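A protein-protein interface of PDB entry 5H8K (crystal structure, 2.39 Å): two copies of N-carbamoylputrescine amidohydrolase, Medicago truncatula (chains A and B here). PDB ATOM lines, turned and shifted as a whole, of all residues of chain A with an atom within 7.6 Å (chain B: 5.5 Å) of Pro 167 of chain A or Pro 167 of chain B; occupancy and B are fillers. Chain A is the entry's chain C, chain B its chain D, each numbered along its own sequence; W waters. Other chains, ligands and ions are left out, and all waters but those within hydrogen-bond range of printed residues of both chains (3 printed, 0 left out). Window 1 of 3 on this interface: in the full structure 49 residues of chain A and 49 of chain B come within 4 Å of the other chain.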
ATOM      1  N   HIS A 126      -1.048  22.995 -18.737  1.00  0.00           N
ATOM      2  CA  HIS A 126       0.302  23.385 -19.123  1.00  0.00           C
ATOM      3  C   HIS A 126       0.915  22.343 -20.057  1.00  0.00           C
ATOM      4  O   HIS A 126       1.008  21.172 -19.699  1.00  0.00           O
ATOM      5  CB  HIS A 126       1.200  23.532 -17.870  1.00  0.00           C
ATOM      6  CG  HIS A 126       0.597  24.363 -16.776  1.00  0.00           C
ATOM      7  ND1 HIS A 126      -0.202  23.823 -15.804  1.00  0.00           N
ATOM      8  CD2 HIS A 126       0.700  25.683 -16.489  1.00  0.00           C
ATOM      9  CE1 HIS A 126      -0.559  24.771 -14.953  1.00  0.00           C
ATOM     10  NE2 HIS A 126      -0.015  25.906 -15.335  1.00  0.00           N
ATOM     11  N   ASP A 163       1.954  19.717 -15.619  1.00  0.00           N
ATOM     12  CA  ASP A 163       1.220  20.548 -14.637  1.00  0.00           C
ATOM     13  C   ASP A 163       1.942  20.554 -13.283  1.00  0.00           C
ATOM     14  O   ASP A 163       1.841  21.491 -12.474  1.00  0.00           O
ATOM     15  CB  ASP A 163      -0.189  20.030 -14.395  1.00  0.00           C
ATOM     16  CG  ASP A 163      -1.177  20.313 -15.525  1.00  0.00           C
ATOM     17  OD1 ASP A 163      -1.032  21.346 -16.221  1.00  0.00           O
ATOM     18  OD2 ASP A 163      -2.154  19.511 -15.669  1.00  0.00           O
ATOM     19  N   GLN A 164       2.665  19.491 -13.024  1.00  0.00           N
ATOM     20  CA  GLN A 164       3.200  19.281 -11.673  1.00  0.00           C
ATOM     21  C   GLN A 164       4.331  20.248 -11.382  1.00  0.00           C
ATOM     22  O   GLN A 164       4.759  20.337 -10.253  1.00  0.00           O
ATOM     23  CB  GLN A 164       3.709  17.837 -11.532  1.00  0.00           C
ATOM     24  CG  GLN A 164       5.027  17.545 -12.273  1.00  0.00           C
ATOM     25  CD  GLN A 164       5.112  16.130 -12.862  1.00  0.00           C
ATOM     26  OE1 GLN A 164       5.680  15.926 -13.959  1.00  0.00           O
ATOM     27  NE2 GLN A 164       4.623  15.133 -12.113  1.00  0.00           N
ATOM     28  N   TRP A 165       4.832  20.969 -12.386  1.00  0.00           N
ATOM     29  CA  TRP A 165       5.913  21.916 -12.139  1.00  0.00           C
ATOM     30  C   TRP A 165       5.390  23.319 -11.697  1.00  0.00           C
ATOM     31  O   TRP A 165       6.183  24.249 -11.376  1.00  0.00           O
ATOM     32  CB  TRP A 165       6.752  22.066 -13.404  1.00  0.00           C
ATOM     33  CG  TRP A 165       7.555  20.841 -13.765  1.00  0.00           C
ATOM     34  CD1 TRP A 165       7.131  19.769 -14.498  1.00  0.00           C
ATOM     35  CD2 TRP A 165       8.932  20.570 -13.394  1.00  0.00           C
ATOM     36  NE1 TRP A 165       8.165  18.828 -14.599  1.00  0.00           N
ATOM     37  CE2 TRP A 165       9.284  19.319 -13.968  1.00  0.00           C
ATOM     38  CE3 TRP A 165       9.917  21.307 -12.729  1.00  0.00           C
ATOM     39  CZ2 TRP A 165      10.556  18.775 -13.854  1.00  0.00           C
ATOM     40  CZ3 TRP A 165      11.170  20.761 -12.585  1.00  0.00           C
ATOM     41  CH2 TRP A 165      11.481  19.476 -13.124  1.00  0.00           C
ATOM     42  N   PHE A 166       4.063  23.468 -11.712  1.00  0.00           N
ATOM     43  CA  PHE A 166       3.421  24.775 -11.533  1.00  0.00           C
ATOM     44  C   PHE A 166       2.741  24.889 -10.181  1.00  0.00           C
ATOM     45  O   PHE A 166       1.690  24.256  -9.952  1.00  0.00           O
ATOM     46  CB  PHE A 166       2.398  24.985 -12.670  1.00  0.00           C
ATOM     47  CG  PHE A 166       3.044  25.123 -13.979  1.00  0.00           C
ATOM     48  CD1 PHE A 166       3.330  24.009 -14.709  1.00  0.00           C
ATOM     49  CD2 PHE A 166       3.480  26.349 -14.394  1.00  0.00           C
ATOM     50  CE1 PHE A 166       3.996  24.100 -15.914  1.00  0.00           C
ATOM     51  CE2 PHE A 166       4.167  26.502 -15.555  1.00  0.00           C
ATOM     52  CZ  PHE A 166       4.415  25.361 -16.345  1.00  0.00           C
ATOM     53  N   PRO A 167       3.316  25.690  -9.289  1.00  0.00           N
ATOM     54  CA  PRO A 167       2.718  25.912  -7.976  1.00  0.00           C
ATOM     55  C   PRO A 167       1.262  26.367  -8.048  1.00  0.00           C
ATOM     56  O   PRO A 167       0.467  25.977  -7.238  1.00  0.00           O
ATOM     57  CB  PRO A 167       3.617  27.024  -7.376  1.00  0.00           C
ATOM     58  CG  PRO A 167       4.952  26.707  -7.975  1.00  0.00           C
ATOM     59  CD  PRO A 167       4.621  26.354  -9.389  1.00  0.00           C
ATOM     60  N   GLU A 168       0.945  27.181  -9.046  1.00  0.00           N
ATOM     61  CA  GLU A 168      -0.416  27.705  -9.258  1.00  0.00           C
ATOM     62  C   GLU A 168      -1.456  26.575  -9.334  1.00  0.00           C
ATOM     63  O   GLU A 168      -2.588  26.694  -8.825  1.00  0.00           O
ATOM     64  CB  GLU A 168      -0.432  28.558 -10.545  1.00  0.00           C
ATOM     65  CG  GLU A 168       0.363  29.864 -10.508  1.00  0.00           C
ATOM     66  CD  GLU A 168       1.803  29.744 -10.991  1.00  0.00           C
ATOM     67  OE1 GLU A 168       2.366  28.627 -10.942  1.00  0.00           O
ATOM     68  OE2 GLU A 168       2.362  30.768 -11.443  1.00  0.00           O
ATOM     69  N   ALA A 169      -1.062  25.443  -9.929  1.00  0.00           N
ATOM     70  CA  ALA A 169      -2.033  24.338 -10.102  1.00  0.00           C
ATOM     71  C   ALA A 169      -2.324  23.629  -8.817  1.00  0.00           C
ATOM     72  O   ALA A 169      -3.486  23.280  -8.564  1.00  0.00           O
ATOM     73  CB  ALA A 169      -1.543  23.304 -11.128  1.00  0.00           C
ATOM     74  N   ALA A 170      -1.268  23.335  -8.036  1.00  0.00           N
ATOM     75  CA  ALA A 170      -1.461  22.686  -6.756  1.00  0.00           C
ATOM     76  C   ALA A 170      -2.291  23.560  -5.867  1.00  0.00           C
ATOM     77  O   ALA A 170      -3.162  23.101  -5.186  1.00  0.00           O
ATOM     78  CB  ALA A 170      -0.123  22.430  -6.098  1.00  0.00           C
ATOM     79  N   ARG A 171      -2.007  24.848  -5.871  1.00  0.00           N
ATOM     80  CA  ARG A 171      -2.708  25.740  -4.975  1.00  0.00           C
ATOM     81  C   ARG A 171      -4.158  25.855  -5.415  1.00  0.00           C
ATOM     82  O   ARG A 171      -5.066  25.851  -4.621  1.00  0.00           O
ATOM     83  CB  ARG A 171      -2.055  27.125  -4.946  1.00  0.00           C
ATOM     84  CG  ARG A 171      -2.846  28.115  -4.068  1.00  0.00           C
ATOM     85  CD  ARG A 171      -2.559  27.867  -2.571  1.00  0.00           C
ATOM     86  NE  ARG A 171      -1.551  28.765  -2.042  1.00  0.00           N
ATOM     87  CZ  ARG A 171      -0.778  28.498  -0.978  1.00  0.00           C
ATOM     88  NH1 ARG A 171      -0.843  27.331  -0.389  1.00  0.00           N
ATOM     89  NH2 ARG A 171       0.053  29.396  -0.538  1.00  0.00           N
ATOM     90  N   ALA A 172      -4.383  25.926  -6.696  1.00  0.00           N
ATOM     91  CA  ALA A 172      -5.776  26.094  -7.178  1.00  0.00           C
ATOM     92  C   ALA A 172      -6.606  24.892  -6.767  1.00  0.00           C
ATOM     93  O   ALA A 172      -7.811  25.015  -6.441  1.00  0.00           O
ATOM     94  CB  ALA A 172      -5.807  26.213  -8.703  1.00  0.00           C
ATOM     95  N   MET A 173      -5.974  23.708  -6.811  1.00  0.00           N
ATOM     96  CA  MET A 173      -6.727  22.531  -6.417  1.00  0.00           C
ATOM     97  C   MET A 173      -6.955  22.569  -4.906  1.00  0.00           C
ATOM     98  O   MET A 173      -8.036  22.267  -4.397  1.00  0.00           O
ATOM     99  CB  MET A 173      -6.055  21.256  -6.903  1.00  0.00           C
ATOM    100  CG  MET A 173      -6.230  21.082  -8.412  1.00  0.00           C
ATOM    101  SD  MET A 173      -5.438  19.577  -9.006  1.00  0.00           S
ATOM    102  CE  MET A 173      -3.679  20.031  -8.932  1.00  0.00           C
ATOM    103  N   TYR A 183      -0.605  13.265  -9.709  1.00  0.00           N
ATOM    104  CA  TYR A 183       0.058  13.622 -10.960  1.00  0.00           C
ATOM    105  C   TYR A 183       0.617  12.385 -11.731  1.00  0.00           C
ATOM    106  O   TYR A 183       1.715  11.949 -11.513  1.00  0.00           O
ATOM    107  CB  TYR A 183       1.179  14.593 -10.670  1.00  0.00           C
ATOM    108  CG  TYR A 183       0.803  15.920 -10.051  1.00  0.00           C
ATOM    109  CD1 TYR A 183       0.496  17.026 -10.860  1.00  0.00           C
ATOM    110  CD2 TYR A 183       0.802  16.099  -8.679  1.00  0.00           C
ATOM    111  CE1 TYR A 183       0.195  18.256 -10.319  1.00  0.00           C
ATOM    112  CE2 TYR A 183       0.480  17.346  -8.117  1.00  0.00           C
ATOM    113  CZ  TYR A 183       0.192  18.414  -8.938  1.00  0.00           C
ATOM    114  OH  TYR A 183      -0.085  19.658  -8.414  1.00  0.00           O
ATOM    115  N   VAL A 205      10.310  20.088  -6.627  1.00  0.00           N
ATOM    116  CA  VAL A 205       9.265  21.050  -6.916  1.00  0.00           C
ATOM    117  C   VAL A 205       7.909  20.554  -6.414  1.00  0.00           C
ATOM    118  O   VAL A 205       7.146  21.321  -5.821  1.00  0.00           O
ATOM    119  CB  VAL A 205       9.214  21.358  -8.424  1.00  0.00           C
ATOM    120  CG1 VAL A 205       7.950  22.131  -8.767  1.00  0.00           C
ATOM    121  CG2 VAL A 205      10.465  22.156  -8.821  1.00  0.00           C
ATOM    122  N   GLY A 208       7.578  20.536  -2.795  1.00  0.00           N
ATOM    123  CA  GLY A 208       7.319  21.872  -2.395  1.00  0.00           C
ATOM    124  C   GLY A 208       5.820  22.132  -2.440  1.00  0.00           C
ATOM    125  O   GLY A 208       5.334  22.896  -1.626  1.00  0.00           O
ATOM    126  N   HIS A 209       5.098  21.520  -3.374  1.00  0.00           N
ATOM    127  CA  HIS A 209       3.627  21.775  -3.475  1.00  0.00           C
ATOM    128  C   HIS A 209       2.964  21.095  -2.297  1.00  0.00           C
ATOM    129  O   HIS A 209       2.042  21.632  -1.691  1.00  0.00           O
ATOM    130  CB  HIS A 209       2.951  21.199  -4.750  1.00  0.00           C
ATOM    131  CG  HIS A 209       3.549  21.655  -6.042  1.00  0.00           C
ATOM    132  ND1 HIS A 209       4.181  22.875  -6.193  1.00  0.00           N
ATOM    133  CD2 HIS A 209       3.634  21.038  -7.235  1.00  0.00           C
ATOM    134  CE1 HIS A 209       4.634  22.984  -7.422  1.00  0.00           C
ATOM    135  NE2 HIS A 209       4.313  21.883  -8.075  1.00  0.00           N
ATOM    136  N   GLY A 211       4.255  20.524   0.613  1.00  0.00           N
ATOM    137  CA  GLY A 211       4.508  21.229   1.895  1.00  0.00           C
ATOM    138  C   GLY A 211       3.824  22.565   2.027  1.00  0.00           C
ATOM    139  O   GLY A 211       3.468  22.992   3.105  1.00  0.00           O
ATOM    140  N   ALA A 212       3.579  23.206   0.899  1.00  0.00           N
ATOM    141  CA  ALA A 212       3.010  24.587   0.907  1.00  0.00           C
ATOM    142  C   ALA A 212       1.492  24.584   1.054  1.00  0.00           C
ATOM    143  O   ALA A 212       0.875  25.586   1.512  1.00  0.00           O
ATOM    144  CB  ALA A 212       3.399  25.318  -0.377  1.00  0.00           C
ATOM    145  N   ASN A 213       0.901  23.476   0.643  1.00  0.00           N
ATOM    146  CA  ASN A 213      -0.530  23.286   0.753  1.00  0.00           C
ATOM    147  C   ASN A 213      -0.924  22.324   1.877  1.00  0.00           C
ATOM    148  O   ASN A 213      -2.113  22.196   2.156  1.00  0.00           O
ATOM    149  CB  ASN A 213      -1.043  22.771  -0.563  1.00  0.00           C
ATOM    150  CG  ASN A 213      -0.958  23.808  -1.626  1.00  0.00           C
ATOM    151  OD1 ASN A 213      -1.718  24.773  -1.601  1.00  0.00           O
ATOM    152  ND2 ASN A 213      -0.006  23.671  -2.541  1.00  0.00           N
ATOM    153  N   VAL A 282      -1.362  28.739   6.753  1.00  0.00           N
ATOM    154  CA  VAL A 282      -0.992  29.455   5.567  1.00  0.00           C
ATOM    155  C   VAL A 282      -2.243  29.956   4.796  1.00  0.00           C
ATOM    156  O   VAL A 282      -2.205  31.070   4.226  1.00  0.00           O
ATOM    157  CB  VAL A 282      -0.055  28.668   4.654  1.00  0.00           C
ATOM    158  CG1 VAL A 282       1.333  28.606   5.265  1.00  0.00           C
ATOM    159  CG2 VAL A 282      -0.580  27.277   4.351  1.00  0.00           C
ATOM    160  N   ARG A 286      -3.020  33.927   3.548  1.00  0.00           N
ATOM    161  CA  ARG A 286      -2.799  34.291   2.138  1.00  0.00           C
ATOM    162  C   ARG A 286      -3.357  35.680   1.827  1.00  0.00           C
ATOM    163  O   ARG A 286      -4.282  36.184   2.507  1.00  0.00           O
ATOM    164  CB  ARG A 286      -3.432  33.265   1.174  1.00  0.00           C
ATOM    165  CG  ARG A 286      -2.741  31.892   1.095  1.00  0.00           C
ATOM    166  CD  ARG A 286      -3.429  30.896   0.156  1.00  0.00           C
ATOM    167  NE  ARG A 286      -3.341  31.344  -1.232  1.00  0.00           N
ATOM    168  CZ  ARG A 286      -4.322  31.989  -1.887  1.00  0.00           C
ATOM    169  NH1 ARG A 286      -5.472  32.174  -1.321  1.00  0.00           N
ATOM    170  NH2 ARG A 286      -4.148  32.351  -3.142  1.00  0.00           N
ATOM    171  N   TYR A 291      -1.950  39.324  -5.133  1.00  0.00           N
ATOM    172  CA  TYR A 291      -1.537  38.364  -6.152  1.00  0.00           C
ATOM    173  C   TYR A 291      -1.919  38.634  -7.622  1.00  0.00           C
ATOM    174  O   TYR A 291      -1.733  37.744  -8.429  1.00  0.00           O
ATOM    175  CB  TYR A 291      -2.046  36.955  -5.800  1.00  0.00           C
ATOM    176  CG  TYR A 291      -1.616  36.424  -4.431  1.00  0.00           C
ATOM    177  CD1 TYR A 291      -0.501  36.908  -3.766  1.00  0.00           C
ATOM    178  CD2 TYR A 291      -2.349  35.425  -3.816  1.00  0.00           C
ATOM    179  CE1 TYR A 291      -0.115  36.384  -2.508  1.00  0.00           C
ATOM    180  CE2 TYR A 291      -1.983  34.914  -2.565  1.00  0.00           C
ATOM    181  CZ  TYR A 291      -0.869  35.382  -1.919  1.00  0.00           C
ATOM    182  OH  TYR A 291      -0.597  34.858  -0.694  1.00  0.00           O
ATOM    183  N   LEU A 294       0.134  37.518 -10.595  1.00  0.00           N
ATOM    184  CA  LEU A 294       0.128  36.178 -11.120  1.00  0.00           C
ATOM    185  C   LEU A 294      -0.750  35.994 -12.350  1.00  0.00           C
ATOM    186  O   LEU A 294      -0.603  34.999 -13.048  1.00  0.00           O
ATOM    187  CB  LEU A 294      -0.316  35.189 -10.070  1.00  0.00           C
ATOM    188  CG  LEU A 294       0.388  35.287  -8.710  1.00  0.00           C
ATOM    189  CD1 LEU A 294      -0.162  34.190  -7.839  1.00  0.00           C
ATOM    190  CD2 LEU A 294       1.852  35.106  -8.865  1.00  0.00           C
ATOM    191  N   ASP B 163       6.650  35.026   4.771  1.00  0.00           N
ATOM    192  CA  ASP B 163       6.410  35.098   3.330  1.00  0.00           C
ATOM    193  C   ASP B 163       6.977  33.887   2.589  1.00  0.00           C
ATOM    194  O   ASP B 163       6.473  33.462   1.508  1.00  0.00           O
ATOM    195  CB  ASP B 163       7.027  36.347   2.724  1.00  0.00           C
ATOM    196  CG  ASP B 163       6.252  37.621   3.027  1.00  0.00           C
ATOM    197  OD1 ASP B 163       5.031  37.546   3.248  1.00  0.00           O
ATOM    198  OD2 ASP B 163       6.876  38.705   3.008  1.00  0.00           O
ATOM    199  N   TRP B 165       6.815  30.830   3.103  1.00  0.00           N
ATOM    200  CA  TRP B 165       5.964  29.659   2.936  1.00  0.00           C
ATOM    201  C   TRP B 165       5.017  29.746   1.709  1.00  0.00           C
ATOM    202  O   TRP B 165       4.373  28.775   1.370  1.00  0.00           O
ATOM    203  CB  TRP B 165       5.138  29.422   4.217  1.00  0.00           C
ATOM    204  CG  TRP B 165       6.029  29.013   5.418  1.00  0.00           C
ATOM    205  CD1 TRP B 165       6.676  29.854   6.241  1.00  0.00           C
ATOM    206  CD2 TRP B 165       6.398  27.690   5.833  1.00  0.00           C
ATOM    207  NE1 TRP B 165       7.415  29.156   7.187  1.00  0.00           N
ATOM    208  CE2 TRP B 165       7.262  27.822   6.953  1.00  0.00           C
ATOM    209  CE3 TRP B 165       6.061  26.400   5.391  1.00  0.00           C
ATOM    210  CZ2 TRP B 165       7.764  26.758   7.633  1.00  0.00           C
ATOM    211  CZ3 TRP B 165       6.595  25.310   6.077  1.00  0.00           C
ATOM    212  CH2 TRP B 165       7.430  25.515   7.194  1.00  0.00           C
ATOM    213  N   PHE B 166       4.996  30.887   1.027  1.00  0.00           N
ATOM    214  CA  PHE B 166       3.969  31.185   0.013  1.00  0.00           C
ATOM    215  C   PHE B 166       4.534  31.192  -1.427  1.00  0.00           C
ATOM    216  O   PHE B 166       5.228  32.112  -1.824  1.00  0.00           O
ATOM    217  CB  PHE B 166       3.231  32.535   0.357  1.00  0.00           C
ATOM    218  CG  PHE B 166       2.500  32.491   1.685  1.00  0.00           C
ATOM    219  CD1 PHE B 166       3.182  32.734   2.867  1.00  0.00           C
ATOM    220  CD2 PHE B 166       1.183  32.109   1.744  1.00  0.00           C
ATOM    221  CE1 PHE B 166       2.546  32.589   4.082  1.00  0.00           C
ATOM    222  CE2 PHE B 166       0.529  31.978   2.937  1.00  0.00           C
ATOM    223  CZ  PHE B 166       1.212  32.201   4.124  1.00  0.00           C
ATOM    224  N   PRO B 167       4.226  30.150  -2.207  1.00  0.00           N
ATOM    225  CA  PRO B 167       4.681  30.102  -3.594  1.00  0.00           C
ATOM    226  C   PRO B 167       4.287  31.359  -4.311  1.00  0.00           C
ATOM    227  O   PRO B 167       5.065  31.797  -5.183  1.00  0.00           O
ATOM    228  CB  PRO B 167       3.922  28.920  -4.180  1.00  0.00           C
ATOM    229  CG  PRO B 167       3.614  28.045  -3.008  1.00  0.00           C
ATOM    230  CD  PRO B 167       3.369  29.001  -1.871  1.00  0.00           C
ATOM    231  N   GLU B 168       3.121  31.934  -3.954  1.00  0.00           N
ATOM    232  CA  GLU B 168       2.651  33.119  -4.644  1.00  0.00           C
ATOM    233  C   GLU B 168       3.652  34.244  -4.571  1.00  0.00           C
ATOM    234  O   GLU B 168       3.829  35.027  -5.515  1.00  0.00           O
ATOM    235  CB  GLU B 168       1.361  33.612  -4.030  1.00  0.00           C
ATOM    236  CG  GLU B 168       0.161  32.752  -4.285  1.00  0.00           C
ATOM    237  CD  GLU B 168      -0.145  31.783  -3.161  1.00  0.00           C
ATOM    238  OE1 GLU B 168       0.794  31.414  -2.402  1.00  0.00           O
ATOM    239  OE2 GLU B 168      -1.323  31.371  -3.053  1.00  0.00           O
ATOM    240  N   ALA B 169       4.348  34.346  -3.449  1.00  0.00           N
ATOM    241  CA  ALA B 169       5.280  35.460  -3.309  1.00  0.00           C
ATOM    242  C   ALA B 169       6.536  35.261  -4.160  1.00  0.00           C
ATOM    243  O   ALA B 169       6.977  36.179  -4.841  1.00  0.00           O
ATOM    244  CB  ALA B 169       5.628  35.645  -1.860  1.00  0.00           C
ATOM    245  N   ALA B 170       7.086  34.054  -4.158  1.00  0.00           N
ATOM    246  CA  ALA B 170       8.260  33.748  -5.017  1.00  0.00           C
ATOM    247  C   ALA B 170       7.936  33.923  -6.538  1.00  0.00           C
ATOM    248  O   ALA B 170       8.708  34.501  -7.310  1.00  0.00           O
ATOM    249  CB  ALA B 170       8.810  32.350  -4.714  1.00  0.00           C
ATOM    250  N   ARG B 171       6.794  33.428  -6.968  1.00  0.00           N
ATOM    251  CA  ARG B 171       6.398  33.580  -8.359  1.00  0.00           C
ATOM    252  C   ARG B 171       6.235  35.066  -8.690  1.00  0.00           C
ATOM    253  O   ARG B 171       6.636  35.507  -9.777  1.00  0.00           O
ATOM    254  CB  ARG B 171       5.096  32.840  -8.627  1.00  0.00           C
ATOM    255  CG  ARG B 171       4.647  32.861 -10.086  1.00  0.00           C
ATOM    256  CD  ARG B 171       5.577  32.025 -10.966  1.00  0.00           C
ATOM    257  NE  ARG B 171       5.039  30.716 -11.259  1.00  0.00           N
ATOM    258  CZ  ARG B 171       5.760  29.687 -11.648  1.00  0.00           C
ATOM    259  NH1 ARG B 171       7.076  29.786 -11.713  1.00  0.00           N
ATOM    260  NH2 ARG B 171       5.166  28.547 -11.982  1.00  0.00           N
ATOM    261  N   ALA B 172       5.683  35.863  -7.774  1.00  0.00           N
ATOM    262  CA  ALA B 172       5.469  37.281  -8.098  1.00  0.00           C
ATOM    263  C   ALA B 172       6.766  38.014  -8.297  1.00  0.00           C
ATOM    264  O   ALA B 172       6.839  38.889  -9.144  1.00  0.00           O
ATOM    265  CB  ALA B 172       4.661  37.985  -7.033  1.00  0.00           C
ATOM    266  N   HIS B 209      10.218  26.637  -4.236  1.00  0.00           N
ATOM    267  CA  HIS B 209      10.181  27.899  -4.929  1.00  0.00           C
ATOM    268  C   HIS B 209      11.378  28.070  -5.841  1.00  0.00           C
ATOM    269  O   HIS B 209      11.228  28.557  -6.976  1.00  0.00           O
ATOM    270  CB  HIS B 209      10.210  29.099  -3.984  1.00  0.00           C
ATOM    271  CG  HIS B 209       9.221  29.050  -2.872  1.00  0.00           C
ATOM    272  ND1 HIS B 209       8.014  28.389  -2.964  1.00  0.00           N
ATOM    273  CD2 HIS B 209       9.234  29.644  -1.655  1.00  0.00           C
ATOM    274  CE1 HIS B 209       7.332  28.564  -1.846  1.00  0.00           C
ATOM    275  NE2 HIS B 209       8.049  29.326  -1.038  1.00  0.00           N
ATOM    276  N   ALA B 212      10.940  25.871  -8.906  1.00  0.00           N
ATOM    277  CA  ALA B 212       9.740  26.160  -9.772  1.00  0.00           C
ATOM    278  C   ALA B 212       9.927  27.467 -10.565  1.00  0.00           C
ATOM    279  O   ALA B 212       9.431  27.618 -11.680  1.00  0.00           O
ATOM    280  CB  ALA B 212       8.480  26.247  -8.933  1.00  0.00           C
ATOM    281  N   ASN B 213      10.692  28.391 -10.000  1.00  0.00           N
ATOM    282  CA  ASN B 213      11.069  29.607 -10.696  1.00  0.00           C
ATOM    283  C   ASN B 213      12.445  29.605 -11.307  1.00  0.00           C
ATOM    284  O   ASN B 213      12.805  30.525 -12.049  1.00  0.00           O
ATOM    285  CB  ASN B 213      10.931  30.746  -9.736  1.00  0.00           C
ATOM    286  CG  ASN B 213       9.498  30.902  -9.301  1.00  0.00           C
ATOM    287  OD1 ASN B 213       8.695  31.459 -10.063  1.00  0.00           O
ATOM    288  ND2 ASN B 213       9.163  30.461  -8.079  1.00  0.00           N
HETATM  289  O   HOH W   1       6.781  25.426  -2.458  1.00  0.00           O
HETATM  290  O   HOH W   2       1.622  28.104   1.557  1.00  0.00           O
HETATM  291  O   HOH W   3       6.898  26.569 -12.557  1.00  0.00           O
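The guanidinium group of Arg 171 of chain B is in salt-bridge range of the side-chain carboxylate of Glu 168 of chain A, at 2.7 Å. The guanidinium group (NE) of Arg 171 of chain A is in salt-bridge range of the side-chain carboxylate (OE2) of Glu 168 of chain B, 2.8 Å away. The guanidinium group of Arg 286 of chain A is in salt-bridge range of the side-chain carboxylate of Glu 168 of chain B, at 2.7 Å.
The guanidinium group (NH1) of Arg 171 of chain A sits at hydrogen-bond distance from the backbone carbonyl oxygen (O) of Ala 212 of chain A (3.1 Å). The side-chain amide oxygen (OD1) of Asn 213 of chain A sits at hydrogen-bond distance from the guanidinium group (NH1) of Arg 171 of chain A. ND1 of His 209 of chain A lies within hydrogen-bond range of O of Val 205 of chain A (3.4 Å). O of Ala 212 of chain B lies within hydrogen-bond range of NH1 of Arg 171 of chain B, 3.2 Å away. The guanidinium group (NH1) of Arg 171 of chain B sits at hydrogen-bond distance from the side-chain amide oxygen (OD1) of Asn 213 of chain B, 2.9 Å away.
Among the printed residues, pairs that only touch across the chains: Val 282 of chain A with Phe 166 of chain B (3.2 Å), Pro 167 of chain A with Arg 171 of chain B (3.4 Å), Tyr 291 of chain A with Glu 168 of chain B (3.5 Å), Arg 171 of chain A with Pro 167 of chain B (3.6 Å), Phe 166 of chain A with Arg 171 of chain B (3.7 Å), Pro 167 of chain A with Ala 212 of chain B (3.7 Å), Arg 171 of chain A with Phe 166 of chain B (3.7 Å), Pro 167 of chain A with Pro 167 of chain B (3.7 Å), Val 205 of chain A with Ala 212 of chain B (3.7 Å), Arg 286 of chain A with Phe 166 of chain B (3.8 Å), Leu 294 of chain A with Arg 171 of chain B (3.8 Å), Ala 212 of chain A with Pro 167 of chain B (3.8 Å), Leu 294 of chain A with Glu 168 of chain B (3.8 Å), Trp 165 of chain A with Ala 212 of chain B (3.9 Å) and Ala 212 of chain A with Trp 165 of chain B (3.99 Å).
Pro 167 of chain A touches just these residues of chain B: Pro 167, Arg 171 and Ala 212. Of the printed residues of chain B, Tyr 291 of chain A touches Glu 168. Of the printed residues of chain B, Leu 294 of chain A touches Glu 168 and Arg 171. Pro 167 of chain B touches three residues of chain A. The nearest residue of chain A that does not touch Pro 167 of chain B is Gly 208 of chain A (5.6 Å).
Of the 12 printed residues of chain B, 6 touch a printed residue of chain A. Hydrophobic or aromatic side chains of chain B within 4 Å of the printed part of chain A: Phe 166, Pro 167 and Ala 212. Of the 23 printed residues of chain A, 11 touch a printed residue of chain B. Printed residues of chain A that touch a printed residue of chain B: Trp 165, Phe 166, Pro 167, Glu 168, Arg 171, Val 205, Ala 212, Val 282, Arg 286, Tyr 291 and Leu 294. Hydrophobic or aromatic side chains of chain A within 4 Å of the printed part of chain B: Phe 166, Pro 167, Val 205, Ala 212, Val 282, Tyr 291 and Leu 294. Among the printed residues, Asp or Glu carboxylates within 4 Å of a Lys or Arg side-chain nitrogen of the other chain: Glu 168 of chain A with Arg 171 of chain B (2.7 Å), Arg 171 of chain A with Glu 168 of chain B (2.8 Å) and Arg 286 of chain A with Glu 168 of chain B (2.7 Å).
Trp 165 of chain A touches Ala 212 of chain B, and with the chains exchanged Ala 212 of chain A touches Trp 165 of chain B. Phe 166 of chain A touches Arg 171 of chain B, and with the chains exchanged Arg 171 of chain A touches Phe 166 of chain B. Pro 167 of chain A touches Arg 171 of chain B, and with the chains exchanged Arg 171 of chain A touches Pro 167 of chain B. Pro 167 of chain A touches Ala 212 of chain B, and with the chains exchanged Ala 212 of chain A touches Pro 167 of chain B. Of the 18 pairs that touch across the chains among the printed residues, 11 have their exchanged pair printed and touching as well.
Water W2 lies within hydrogen-bond range of the backbone carbonyl oxygen of Ala 212 of chain A (2.6 Å), the backbone carbonyl oxygen of Trp 165 of chain B (2.8 Å) and the guanidinium group of Arg 171 of chain A (2.9 Å). Water W3 lies within hydrogen-bond range of NH2 of Arg 171 of chain B (2.7 Å), O of Trp 165 of chain A (2.7 Å) and O of Ala 212 of chain B (2.9 Å). Water W1 bridges the backbone carbonyl oxygen (O) of Gly 208 of chain A (3.0 Å) and a ring nitrogen (ND1) of His 209 of chain B (3.2 Å).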
